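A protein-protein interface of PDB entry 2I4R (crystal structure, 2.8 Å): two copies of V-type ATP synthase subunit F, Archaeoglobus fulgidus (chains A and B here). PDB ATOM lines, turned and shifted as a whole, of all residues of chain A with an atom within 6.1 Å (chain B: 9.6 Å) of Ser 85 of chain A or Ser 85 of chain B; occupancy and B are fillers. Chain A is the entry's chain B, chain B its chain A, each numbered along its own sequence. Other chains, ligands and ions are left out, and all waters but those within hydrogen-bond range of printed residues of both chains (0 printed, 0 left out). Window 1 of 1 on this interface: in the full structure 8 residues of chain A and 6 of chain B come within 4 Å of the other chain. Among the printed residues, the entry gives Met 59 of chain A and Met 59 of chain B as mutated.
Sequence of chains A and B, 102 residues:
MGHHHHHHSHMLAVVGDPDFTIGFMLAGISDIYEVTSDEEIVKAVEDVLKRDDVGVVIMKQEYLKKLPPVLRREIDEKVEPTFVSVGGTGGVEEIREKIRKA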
ATOM      1  N   VAL A  57       2.797  11.509  10.854  1.00  0.00           N
ATOM      2  CA  VAL A  57       1.786  12.474  11.256  1.00  0.00           C
ATOM      3  C   VAL A  57       2.444  13.803  11.588  1.00  0.00           C
ATOM      4  O   VAL A  57       3.330  13.875  12.430  1.00  0.00           O
ATOM      5  CB  VAL A  57       0.935  11.952  12.462  1.00  0.00           C
ATOM      6  CG1 VAL A  57       1.797  11.144  13.389  1.00  0.00           C
ATOM      7  CG2 VAL A  57       0.276  13.122  13.214  1.00  0.00           C
ATOM      8  N   ILE A  58       2.014  14.843  10.881  1.00  0.00           N
ATOM      9  CA  ILE A  58       2.519  16.205  11.069  1.00  0.00           C
ATOM     10  C   ILE A  58       1.763  16.868  12.216  1.00  0.00           C
ATOM     11  O   ILE A  58       0.546  16.720  12.327  1.00  0.00           O
ATOM     12  CB  ILE A  58       2.275  17.096   9.823  1.00  0.00           C
ATOM     13  CG1 ILE A  58       2.720  16.384   8.544  1.00  0.00           C
ATOM     14  CG2 ILE A  58       3.009  18.412   9.991  1.00  0.00           C
ATOM     15  CD1 ILE A  58       4.206  16.259   8.402  1.00  0.00           C
ATOM     16  N   MET A  59       2.466  17.618  13.053  1.00  0.00           N
ATOM     17  CA  MET A  59       1.814  18.292  14.165  1.00  0.00           C
ATOM     18  C   MET A  59       2.564  19.511  14.660  1.00  0.00           C
ATOM     19  O   MET A  59       3.759  19.663  14.423  1.00  0.00           O
ATOM     20  CB  MET A  59       1.669  17.352  15.351  1.00  0.00           C
ATOM     21  CG  MET A  59       0.411  16.526  15.406  1.00  0.00           C
ATOM     22  SD  MET A  59       0.085  16.143  17.274  1.00  0.00           S
ATOM     23  CE  MET A  59       1.739  15.215  17.703  1.00  0.00           C
ATOM     24  N   LYS A  60       1.846  20.373  15.370  1.00  0.00           N
ATOM     25  CA  LYS A  60       2.447  21.557  15.944  1.00  0.00           C
ATOM     26  C   LYS A  60       3.315  21.052  17.089  1.00  0.00           C
ATOM     27  O   LYS A  60       2.916  20.163  17.839  1.00  0.00           O
ATOM     28  CB  LYS A  60       1.361  22.492  16.469  1.00  0.00           C
ATOM     29  CG  LYS A  60       0.546  23.160  15.379  1.00  0.00           C
ATOM     30  CD  LYS A  60       0.976  24.617  15.171  1.00  0.00           C
ATOM     31  CE  LYS A  60      -0.040  25.585  15.769  1.00  0.00           C
ATOM     32  NZ  LYS A  60      -1.393  25.441  15.130  1.00  0.00           N
ATOM     33  N   GLN A  61       4.508  21.614  17.218  1.00  0.00           N
ATOM     34  CA  GLN A  61       5.428  21.195  18.262  1.00  0.00           C
ATOM     35  C   GLN A  61       4.823  21.506  19.618  1.00  0.00           C
ATOM     36  O   GLN A  61       5.235  20.966  20.642  1.00  0.00           O
ATOM     37  CB  GLN A  61       6.754  21.932  18.091  1.00  0.00           C
ATOM     38  CG  GLN A  61       7.957  21.219  18.676  1.00  0.00           C
ATOM     39  CD  GLN A  61       9.268  21.746  18.101  1.00  0.00           C
ATOM     40  OE1 GLN A  61       9.596  22.931  18.244  1.00  0.00           O
ATOM     41  NE2 GLN A  61      10.021  20.869  17.438  1.00  0.00           N
ATOM     42  N   LEU A  64       2.483  18.261  22.069  1.00  0.00           N
ATOM     43  CA  LEU A  64       2.915  17.200  22.978  1.00  0.00           C
ATOM     44  C   LEU A  64       2.648  17.568  24.435  1.00  0.00           C
ATOM     45  O   LEU A  64       2.154  16.748  25.208  1.00  0.00           O
ATOM     46  CB  LEU A  64       4.409  16.905  22.819  1.00  0.00           C
ATOM     47  CG  LEU A  64       4.931  16.305  21.518  1.00  0.00           C
ATOM     48  CD1 LEU A  64       5.050  17.405  20.478  1.00  0.00           C
ATOM     49  CD2 LEU A  64       6.294  15.649  21.765  1.00  0.00           C
ATOM     50  N   PHE A  83       6.404  10.597  14.078  1.00  0.00           N
ATOM     51  CA  PHE A  83       5.834  11.916  14.289  1.00  0.00           C
ATOM     52  C   PHE A  83       6.772  12.990  13.769  1.00  0.00           C
ATOM     53  O   PHE A  83       7.990  12.884  13.904  1.00  0.00           O
ATOM     54  CB  PHE A  83       5.527  12.149  15.767  1.00  0.00           C
ATOM     55  CG  PHE A  83       4.244  11.525  16.207  1.00  0.00           C
ATOM     56  CD1 PHE A  83       4.134  10.140  16.326  1.00  0.00           C
ATOM     57  CD2 PHE A  83       3.114  12.307  16.420  1.00  0.00           C
ATOM     58  CE1 PHE A  83       2.909   9.539  16.645  1.00  0.00           C
ATOM     59  CE2 PHE A  83       1.883  11.721  16.739  1.00  0.00           C
ATOM     60  CZ  PHE A  83       1.782  10.331  16.850  1.00  0.00           C
ATOM     61  N   VAL A  84       6.188  14.008  13.147  1.00  0.00           N
ATOM     62  CA  VAL A  84       6.935  15.132  12.594  1.00  0.00           C
ATOM     63  C   VAL A  84       6.331  16.366  13.267  1.00  0.00           C
ATOM     64  O   VAL A  84       5.137  16.630  13.129  1.00  0.00           O
ATOM     65  CB  VAL A  84       6.747  15.189  11.052  1.00  0.00           C
ATOM     66  CG1 VAL A  84       7.525  16.334  10.449  1.00  0.00           C
ATOM     67  CG2 VAL A  84       7.198  13.896  10.441  1.00  0.00           C
ATOM     68  N   SER A  85       7.139  17.118  14.009  1.00  0.00           N
ATOM     69  CA  SER A  85       6.600  18.280  14.710  1.00  0.00           C
ATOM     70  C   SER A  85       7.050  19.629  14.187  1.00  0.00           C
ATOM     71  O   SER A  85       8.234  19.967  14.215  1.00  0.00           O
ATOM     72  CB  SER A  85       6.922  18.193  16.201  1.00  0.00           C
ATOM     73  OG  SER A  85       8.302  18.411  16.408  1.00  0.00           O
ATOM     74  N   VAL A  86       6.072  20.400  13.732  1.00  0.00           N
ATOM     75  CA  VAL A  86       6.303  21.723  13.189  1.00  0.00           C
ATOM     76  C   VAL A  86       6.702  22.677  14.307  1.00  0.00           C
ATOM     77  O   VAL A  86       5.858  23.147  15.069  1.00  0.00           O
ATOM     78  CB  VAL A  86       5.031  22.253  12.471  1.00  0.00           C
ATOM     79  CG1 VAL A  86       5.280  23.636  11.916  1.00  0.00           C
ATOM     80  CG2 VAL A  86       4.638  21.311  11.348  1.00  0.00           C
ATOM     81  N   GLY A  87       8.003  22.945  14.382  1.00  0.00           N
ATOM     82  CA  GLY A  87       8.568  23.832  15.385  1.00  0.00           C
ATOM     83  C   GLY A  87       7.743  25.051  15.755  1.00  0.00           C
ATOM     84  O   GLY A  87       7.765  25.425  16.952  1.00  0.00           O
ATOM     85  N   ALA B  13      14.350  23.853   3.098  1.00  0.00           N
ATOM     86  CA  ALA B  13      15.678  23.282   3.078  1.00  0.00           C
ATOM     87  C   ALA B  13      15.595  22.032   3.930  1.00  0.00           C
ATOM     88  O   ALA B  13      14.786  21.959   4.858  1.00  0.00           O
ATOM     89  CB  ALA B  13      16.690  24.274   3.653  1.00  0.00           C
ATOM     90  N   VAL B  15      18.039  19.072   5.974  1.00  0.00           N
ATOM     91  CA  VAL B  15      19.353  18.779   6.514  1.00  0.00           C
ATOM     92  C   VAL B  15      19.397  17.330   6.947  1.00  0.00           C
ATOM     93  O   VAL B  15      18.549  16.893   7.723  1.00  0.00           O
ATOM     94  CB  VAL B  15      19.626  19.668   7.750  1.00  0.00           C
ATOM     95  CG1 VAL B  15      21.013  19.404   8.301  1.00  0.00           C
ATOM     96  CG2 VAL B  15      19.462  21.137   7.375  1.00  0.00           C
ATOM     97  N   PHE B  20      18.657   9.959   4.198  1.00  0.00           N
ATOM     98  CA  PHE B  20      17.501  10.703   4.674  1.00  0.00           C
ATOM     99  C   PHE B  20      17.058  11.748   3.662  1.00  0.00           C
ATOM    100  O   PHE B  20      15.872  11.991   3.490  1.00  0.00           O
ATOM    101  CB  PHE B  20      17.825  11.390   5.995  1.00  0.00           C
ATOM    102  CG  PHE B  20      16.751  12.323   6.479  1.00  0.00           C
ATOM    103  CD1 PHE B  20      16.694  13.642   6.033  1.00  0.00           C
ATOM    104  CD2 PHE B  20      15.802  11.891   7.396  1.00  0.00           C
ATOM    105  CE1 PHE B  20      15.703  14.518   6.498  1.00  0.00           C
ATOM    106  CE2 PHE B  20      14.809  12.763   7.864  1.00  0.00           C
ATOM    107  CZ  PHE B  20      14.763  14.076   7.413  1.00  0.00           C
ATOM    108  N   PHE B  24      13.662  13.210  -0.620  1.00  0.00           N
ATOM    109  CA  PHE B  24      13.291  14.606  -0.804  1.00  0.00           C
ATOM    110  C   PHE B  24      13.750  15.127  -2.151  1.00  0.00           C
ATOM    111  O   PHE B  24      13.038  15.881  -2.814  1.00  0.00           O
ATOM    112  CB  PHE B  24      13.887  15.465   0.310  1.00  0.00           C
ATOM    113  CG  PHE B  24      13.332  15.162   1.673  1.00  0.00           C
ATOM    114  CD1 PHE B  24      14.104  14.523   2.626  1.00  0.00           C
ATOM    115  CD2 PHE B  24      12.024  15.508   1.998  1.00  0.00           C
ATOM    116  CE1 PHE B  24      13.580  14.231   3.885  1.00  0.00           C
ATOM    117  CE2 PHE B  24      11.497  15.218   3.253  1.00  0.00           C
ATOM    118  CZ  PHE B  24      12.276  14.580   4.192  1.00  0.00           C
ATOM    119  N   VAL B  56      11.503  27.362   5.773  1.00  0.00           N
ATOM    120  CA  VAL B  56      11.321  26.125   6.521  1.00  0.00           C
ATOM    121  C   VAL B  56      12.476  25.155   6.270  1.00  0.00           C
ATOM    122  O   VAL B  56      13.001  25.053   5.149  1.00  0.00           O
ATOM    123  CB  VAL B  56       9.964  25.434   6.143  1.00  0.00           C
ATOM    124  CG1 VAL B  56       9.917  25.154   4.652  1.00  0.00           C
ATOM    125  CG2 VAL B  56       9.783  24.140   6.921  1.00  0.00           C
ATOM    126  N   VAL B  57      12.873  24.447   7.324  1.00  0.00           N
ATOM    127  CA  VAL B  57      13.951  23.481   7.225  1.00  0.00           C
ATOM    128  C   VAL B  57      13.565  22.175   7.909  1.00  0.00           C
ATOM    129  O   VAL B  57      13.198  22.163   9.079  1.00  0.00           O
ATOM    130  CB  VAL B  57      15.248  24.056   7.852  1.00  0.00           C
ATOM    131  CG1 VAL B  57      14.912  24.743   9.146  1.00  0.00           C
ATOM    132  CG2 VAL B  57      16.284  22.946   8.090  1.00  0.00           C
ATOM    133  N   ILE B  58      13.625  21.086   7.148  1.00  0.00           N
ATOM    134  CA  ILE B  58      13.312  19.752   7.655  1.00  0.00           C
ATOM    135  C   ILE B  58      14.610  19.147   8.176  1.00  0.00           C
ATOM    136  O   ILE B  58      15.662  19.277   7.556  1.00  0.00           O
ATOM    137  CB  ILE B  58      12.735  18.843   6.551  1.00  0.00           C
ATOM    138  CG1 ILE B  58      11.468  19.480   5.977  1.00  0.00           C
ATOM    139  CG2 ILE B  58      12.455  17.449   7.113  1.00  0.00           C
ATOM    140  CD1 ILE B  58      10.837  18.704   4.834  1.00  0.00           C
ATOM    141  N   MET B  59      14.531  18.462   9.307  1.00  0.00           N
ATOM    142  CA  MET B  59      15.725  17.912   9.920  1.00  0.00           C
ATOM    143  C   MET B  59      15.325  16.914  10.999  1.00  0.00           C
ATOM    144  O   MET B  59      14.301  17.090  11.654  1.00  0.00           O
ATOM    145  CB  MET B  59      16.487  19.092  10.513  1.00  0.00           C
ATOM    146  CG  MET B  59      17.764  18.818  11.247  1.00  0.00           C
ATOM    147  SD  MET B  59      18.297  20.502  12.038  1.00  0.00           S
ATOM    148  CE  MET B  59      16.957  20.602  13.447  1.00  0.00           C
ATOM    149  N   LYS B  60      16.120  15.863  11.179  1.00  0.00           N
ATOM    150  CA  LYS B  60      15.811  14.854  12.191  1.00  0.00           C
ATOM    151  C   LYS B  60      15.809  15.422  13.614  1.00  0.00           C
ATOM    152  O   LYS B  60      16.514  16.383  13.923  1.00  0.00           O
ATOM    153  CB  LYS B  60      16.794  13.677  12.097  1.00  0.00           C
ATOM    154  CG  LYS B  60      16.139  12.359  11.651  1.00  0.00           C
ATOM    155  CD  LYS B  60      17.126  11.195  11.603  1.00  0.00           C
ATOM    156  CE  LYS B  60      18.211  11.406  10.541  1.00  0.00           C
ATOM    157  NZ  LYS B  60      19.192  10.274  10.490  1.00  0.00           N
ATOM    158  N   GLN B  61      15.003  14.810  14.475  1.00  0.00           N
ATOM    159  CA  GLN B  61      14.875  15.230  15.863  1.00  0.00           C
ATOM    160  C   GLN B  61      16.219  15.103  16.587  1.00  0.00           C
ATOM    161  O   GLN B  61      16.616  15.967  17.371  1.00  0.00           O
ATOM    162  CB  GLN B  61      13.823  14.354  16.545  1.00  0.00           C
ATOM    163  CG  GLN B  61      13.043  15.035  17.655  1.00  0.00           C
ATOM    164  CD  GLN B  61      13.899  15.360  18.866  1.00  0.00           C
ATOM    165  OE1 GLN B  61      14.582  14.483  19.403  1.00  0.00           O
ATOM    166  NE2 GLN B  61      13.862  16.619  19.309  1.00  0.00           N
ATOM    167  N   GLU B  62      16.918  14.016  16.290  1.00  0.00           N
ATOM    168  CA  GLU B  62      18.205  13.708  16.898  1.00  0.00           C
ATOM    169  C   GLU B  62      19.339  14.678  16.587  1.00  0.00           C
ATOM    170  O   GLU B  62      20.487  14.388  16.920  1.00  0.00           O
ATOM    171  CB  GLU B  62      18.645  12.311  16.472  1.00  0.00           C
ATOM    172  CG  GLU B  62      19.025  12.252  15.009  1.00  0.00           C
ATOM    173  CD  GLU B  62      19.366  10.852  14.557  1.00  0.00           C
ATOM    174  OE1 GLU B  62      18.470   9.980  14.621  1.00  0.00           O
ATOM    175  OE2 GLU B  62      20.529  10.628  14.138  1.00  0.00           O
ATOM    176  N   TYR B  63      19.050  15.810  15.953  1.00  0.00           N
ATOM    177  CA  TYR B  63      20.121  16.755  15.643  1.00  0.00           C
ATOM    178  C   TYR B  63      20.240  17.961  16.564  1.00  0.00           C
ATOM    179  O   TYR B  63      21.234  18.678  16.502  1.00  0.00           O
ATOM    180  CB  TYR B  63      20.010  17.251  14.203  1.00  0.00           C
ATOM    181  CG  TYR B  63      20.423  16.234  13.173  1.00  0.00           C
ATOM    182  CD1 TYR B  63      20.555  16.592  11.830  1.00  0.00           C
ATOM    183  CD2 TYR B  63      20.703  14.908  13.540  1.00  0.00           C
ATOM    184  CE1 TYR B  63      20.959  15.659  10.877  1.00  0.00           C
ATOM    185  CE2 TYR B  63      21.109  13.969  12.595  1.00  0.00           C
ATOM    186  CZ  TYR B  63      21.237  14.353  11.267  1.00  0.00           C
ATOM    187  OH  TYR B  63      21.664  13.437  10.335  1.00  0.00           O
ATOM    188  N   LEU B  64      19.245  18.180  17.420  1.00  0.00           N
ATOM    189  CA  LEU B  64      19.266  19.323  18.329  1.00  0.00           C
ATOM    190  C   LEU B  64      20.333  19.200  19.416  1.00  0.00           C
ATOM    191  O   LEU B  64      21.105  20.130  19.644  1.00  0.00           O
ATOM    192  CB  LEU B  64      17.887  19.514  18.957  1.00  0.00           C
ATOM    193  N   ILE B  75      17.292  29.112  17.678  1.00  0.00           N
ATOM    194  CA  ILE B  75      16.081  28.739  16.967  1.00  0.00           C
ATOM    195  C   ILE B  75      15.015  28.778  18.055  1.00  0.00           C
ATOM    196  O   ILE B  75      13.911  28.242  17.911  1.00  0.00           O
ATOM    197  CB  ILE B  75      16.193  27.322  16.355  1.00  0.00           C
ATOM    198  CG1 ILE B  75      16.263  26.266  17.453  1.00  0.00           C
ATOM    199  CG2 ILE B  75      17.460  27.219  15.512  1.00  0.00           C
ATOM    200  CD1 ILE B  75      16.334  24.860  16.914  1.00  0.00           C
ATOM    201  N   LYS B  78      12.757  30.809  16.444  1.00  0.00           N
ATOM    202  CA  LYS B  78      12.218  30.055  15.308  1.00  0.00           C
ATOM    203  C   LYS B  78      11.260  30.961  14.516  1.00  0.00           C
ATOM    204  O   LYS B  78      10.241  30.499  13.992  1.00  0.00           O
ATOM    205  CB  LYS B  78      11.457  28.817  15.786  1.00  0.00           C
ATOM    206  CG  LYS B  78      12.177  27.515  15.478  1.00  0.00           C
ATOM    207  CD  LYS B  78      11.295  26.315  15.777  1.00  0.00           C
ATOM    208  CE  LYS B  78      12.127  25.053  15.969  1.00  0.00           C
ATOM    209  NZ  LYS B  78      12.922  25.096  17.229  1.00  0.00           N
ATOM    210  N   THR B  82      10.939  28.377  10.107  1.00  0.00           N
ATOM    211  CA  THR B  82      10.369  27.435  11.059  1.00  0.00           C
ATOM    212  C   THR B  82      11.107  26.072  10.850  1.00  0.00           C
ATOM    213  O   THR B  82      11.355  25.640   9.717  1.00  0.00           O
ATOM    214  CB  THR B  82       8.865  27.210  10.847  1.00  0.00           C
ATOM    215  OG1 THR B  82       8.207  28.467  10.974  1.00  0.00           O
ATOM    216  CG2 THR B  82       8.292  26.345  11.950  1.00  0.00           C
ATOM    217  N   PHE B  83      11.463  25.427  11.958  1.00  0.00           N
ATOM    218  CA  PHE B  83      12.126  24.133  11.904  1.00  0.00           C
ATOM    219  C   PHE B  83      11.100  23.011  12.054  1.00  0.00           C
ATOM    220  O   PHE B  83      10.125  23.147  12.793  1.00  0.00           O
ATOM    221  CB  PHE B  83      13.208  24.046  12.982  1.00  0.00           C
ATOM    222  CG  PHE B  83      14.480  24.764  12.606  1.00  0.00           C
ATOM    223  CD1 PHE B  83      14.487  26.142  12.414  1.00  0.00           C
ATOM    224  CD2 PHE B  83      15.664  24.053  12.391  1.00  0.00           C
ATOM    225  CE1 PHE B  83      15.655  26.803  12.011  1.00  0.00           C
ATOM    226  CE2 PHE B  83      16.838  24.706  11.986  1.00  0.00           C
ATOM    227  CZ  PHE B  83      16.833  26.079  11.796  1.00  0.00           C
ATOM    228  N   VAL B  84      11.307  21.925  11.312  1.00  0.00           N
ATOM    229  CA  VAL B  84      10.404  20.782  11.339  1.00  0.00           C
ATOM    230  C   VAL B  84      11.227  19.549  11.656  1.00  0.00           C
ATOM    231  O   VAL B  84      11.964  19.064  10.804  1.00  0.00           O
ATOM    232  CB  VAL B  84       9.725  20.578   9.961  1.00  0.00           C
ATOM    233  CG1 VAL B  84       8.858  19.329   9.976  1.00  0.00           C
ATOM    234  CG2 VAL B  84       8.892  21.793   9.603  1.00  0.00           C
ATOM    235  N   SER B  85      11.095  19.032  12.875  1.00  0.00           N
ATOM    236  CA  SER B  85      11.866  17.856  13.273  1.00  0.00           C
ATOM    237  C   SER B  85      11.140  16.532  13.120  1.00  0.00           C
ATOM    238  O   SER B  85      10.002  16.360  13.569  1.00  0.00           O
ATOM    239  CB  SER B  85      12.368  17.999  14.715  1.00  0.00           C
ATOM    240  OG  SER B  85      11.291  18.215  15.605  1.00  0.00           O
ATOM    241  N   VAL B  86      11.832  15.605  12.469  1.00  0.00           N
ATOM    242  CA  VAL B  86      11.332  14.262  12.218  1.00  0.00           C
ATOM    243  C   VAL B  86      11.852  13.356  13.327  1.00  0.00           C
ATOM    244  O   VAL B  86      13.066  13.187  13.465  1.00  0.00           O
ATOM    245  CB  VAL B  86      11.849  13.735  10.863  1.00  0.00           C
ATOM    246  CG1 VAL B  86      11.168  12.425  10.515  1.00  0.00           C
ATOM    247  CG2 VAL B  86      11.628  14.784   9.784  1.00  0.00           C
ATOM    248  N   GLY B  87      10.938  12.776  14.109  1.00  0.00           N
ATOM    249  CA  GLY B  87      11.337  11.906  15.205  1.00  0.00           C
ATOM    250  C   GLY B  87      11.787  10.508  14.797  1.00  0.00           C
ATOM    251  O   GLY B  87      11.715   9.581  15.642  1.00  0.00           O
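The side-chain amide nitrogen of Gln 61 of chain A is in hydrogen-bond range of the side-chain hydroxyl of Ser 85 of chain B (3.5 Å).
N of Ser 85 of chain A lies within hydrogen-bond range of O of Ser 85 of chain B (3.0 Å).
O of Phe 83 of chain A lies within hydrogen-bond range of N of Gly 87 of chain B, 3.0 Å away.
The backbone carbonyl oxygen of Phe 83 of chain B sits at hydrogen-bond distance from the backbone NH of Gly 87 of chain A (2.7 Å).
Phe 83 of chain A touches Gly 87 of chain B, and with the chains exchanged Gly 87 of chain A touches Phe 83 of chain B.
Val 84 of chain B touches its own counterpart, Val 84 of chain A.
Ser 85 of chain A touches Phe 83 of chain B, but with the chains exchanged Phe 83 of chain A does not touch Ser 85 of chain B (4.03 Å).
Ser 85 of chain B touches its own counterpart, Ser 85 of chain A.
Of the 11 pairs that touch across the chains among the printed residues, 8 have their exchanged pair printed and touching as well.
Of chain A, only Gln 61, Val 84 and Ser 85 come within 4 Å of Ser 85 of chain B.
Of the printed residues of chain B, Val 84 of chain A touches Val 84 and Ser 85.
Of chain B, only Phe 83 comes within 4 Å of Val 86 of chain A.
Of the printed residues of chain A, Lys 78 of chain B touches Gly 87.
Printed residues of chain A within 4 Å of Val 84 of chain B: Val 84 (3.3 Å) and Ser 85 (3.7 Å).
Of the printed residues of chain B, Gly 87 of chain A touches Lys 78 (3.7 Å) and Phe 83 (2.7 Å).
Printed residues of chain B within 4 Å of Phe 83 of chain A: Val 86 and Gly 87.
Leu 64 of chain A touches none of the printed residues of chain B.
Met 59 of chain A touches none of the printed residues of chain B.
The nearest residue of chain B that does not touch Ser 85 of chain A is Val 86 of chain B (5.2 Å).
The nearest printed residue of chain B that does not touch Phe 83 of chain A is Ser 85 of chain B (4.03 Å).
Among the printed residues, pairs that only touch across the chains: Val 84 of chain A with Val 84 of chain B, Val 84 of chain A with Ser 85 of chain B, Ser 85 of chain A with Val 84 of chain B, Gly 87 of chain A with Lys 78 of chain B, Val 86 of chain A with Phe 83 of chain B, Phe 83 of chain A with Val 86 of chain B and Ser 85 of chain A with Phe 83 of chain B.
Printed residues of chain A that touch a printed residue of chain B: Gln 61, Phe 83, Val 84, Ser 85, Val 86 and Gly 87.
Among the printed residues, no Asp or Glu carboxylate lies within 4 Å of a Lys or Arg side-chain nitrogen of the other chain.
The side-chain amide oxygen (OE1) of Gln 61 of chain A sits close to the backbone carbonyl oxygen (O) of Gly 87 of chain A (3.4 Å).
O of Val 57 of chain A sits at hydrogen-bond distance from N of Val 84 of chain A (2.9 Å).
The backbone NH (N) of Val 84 of chain B is in hydrogen-bond range of the backbone carbonyl oxygen (O) of Val 57 of chain B (2.9 Å).
The backbone NH (N) of Val 86 of chain A sits at hydrogen-bond distance from the backbone carbonyl oxygen (O) of Met 59 of chain A (2.5 Å).
The backbone carbonyl oxygen (O) of Ile 75 of chain B lies close to the side-chain amino group (NZ) of Lys 78 of chain B, 3.4 Å away.
N of Val 86 of chain B sits at hydrogen-bond distance from O of Met 59 of chain B, at 3.0 Å.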
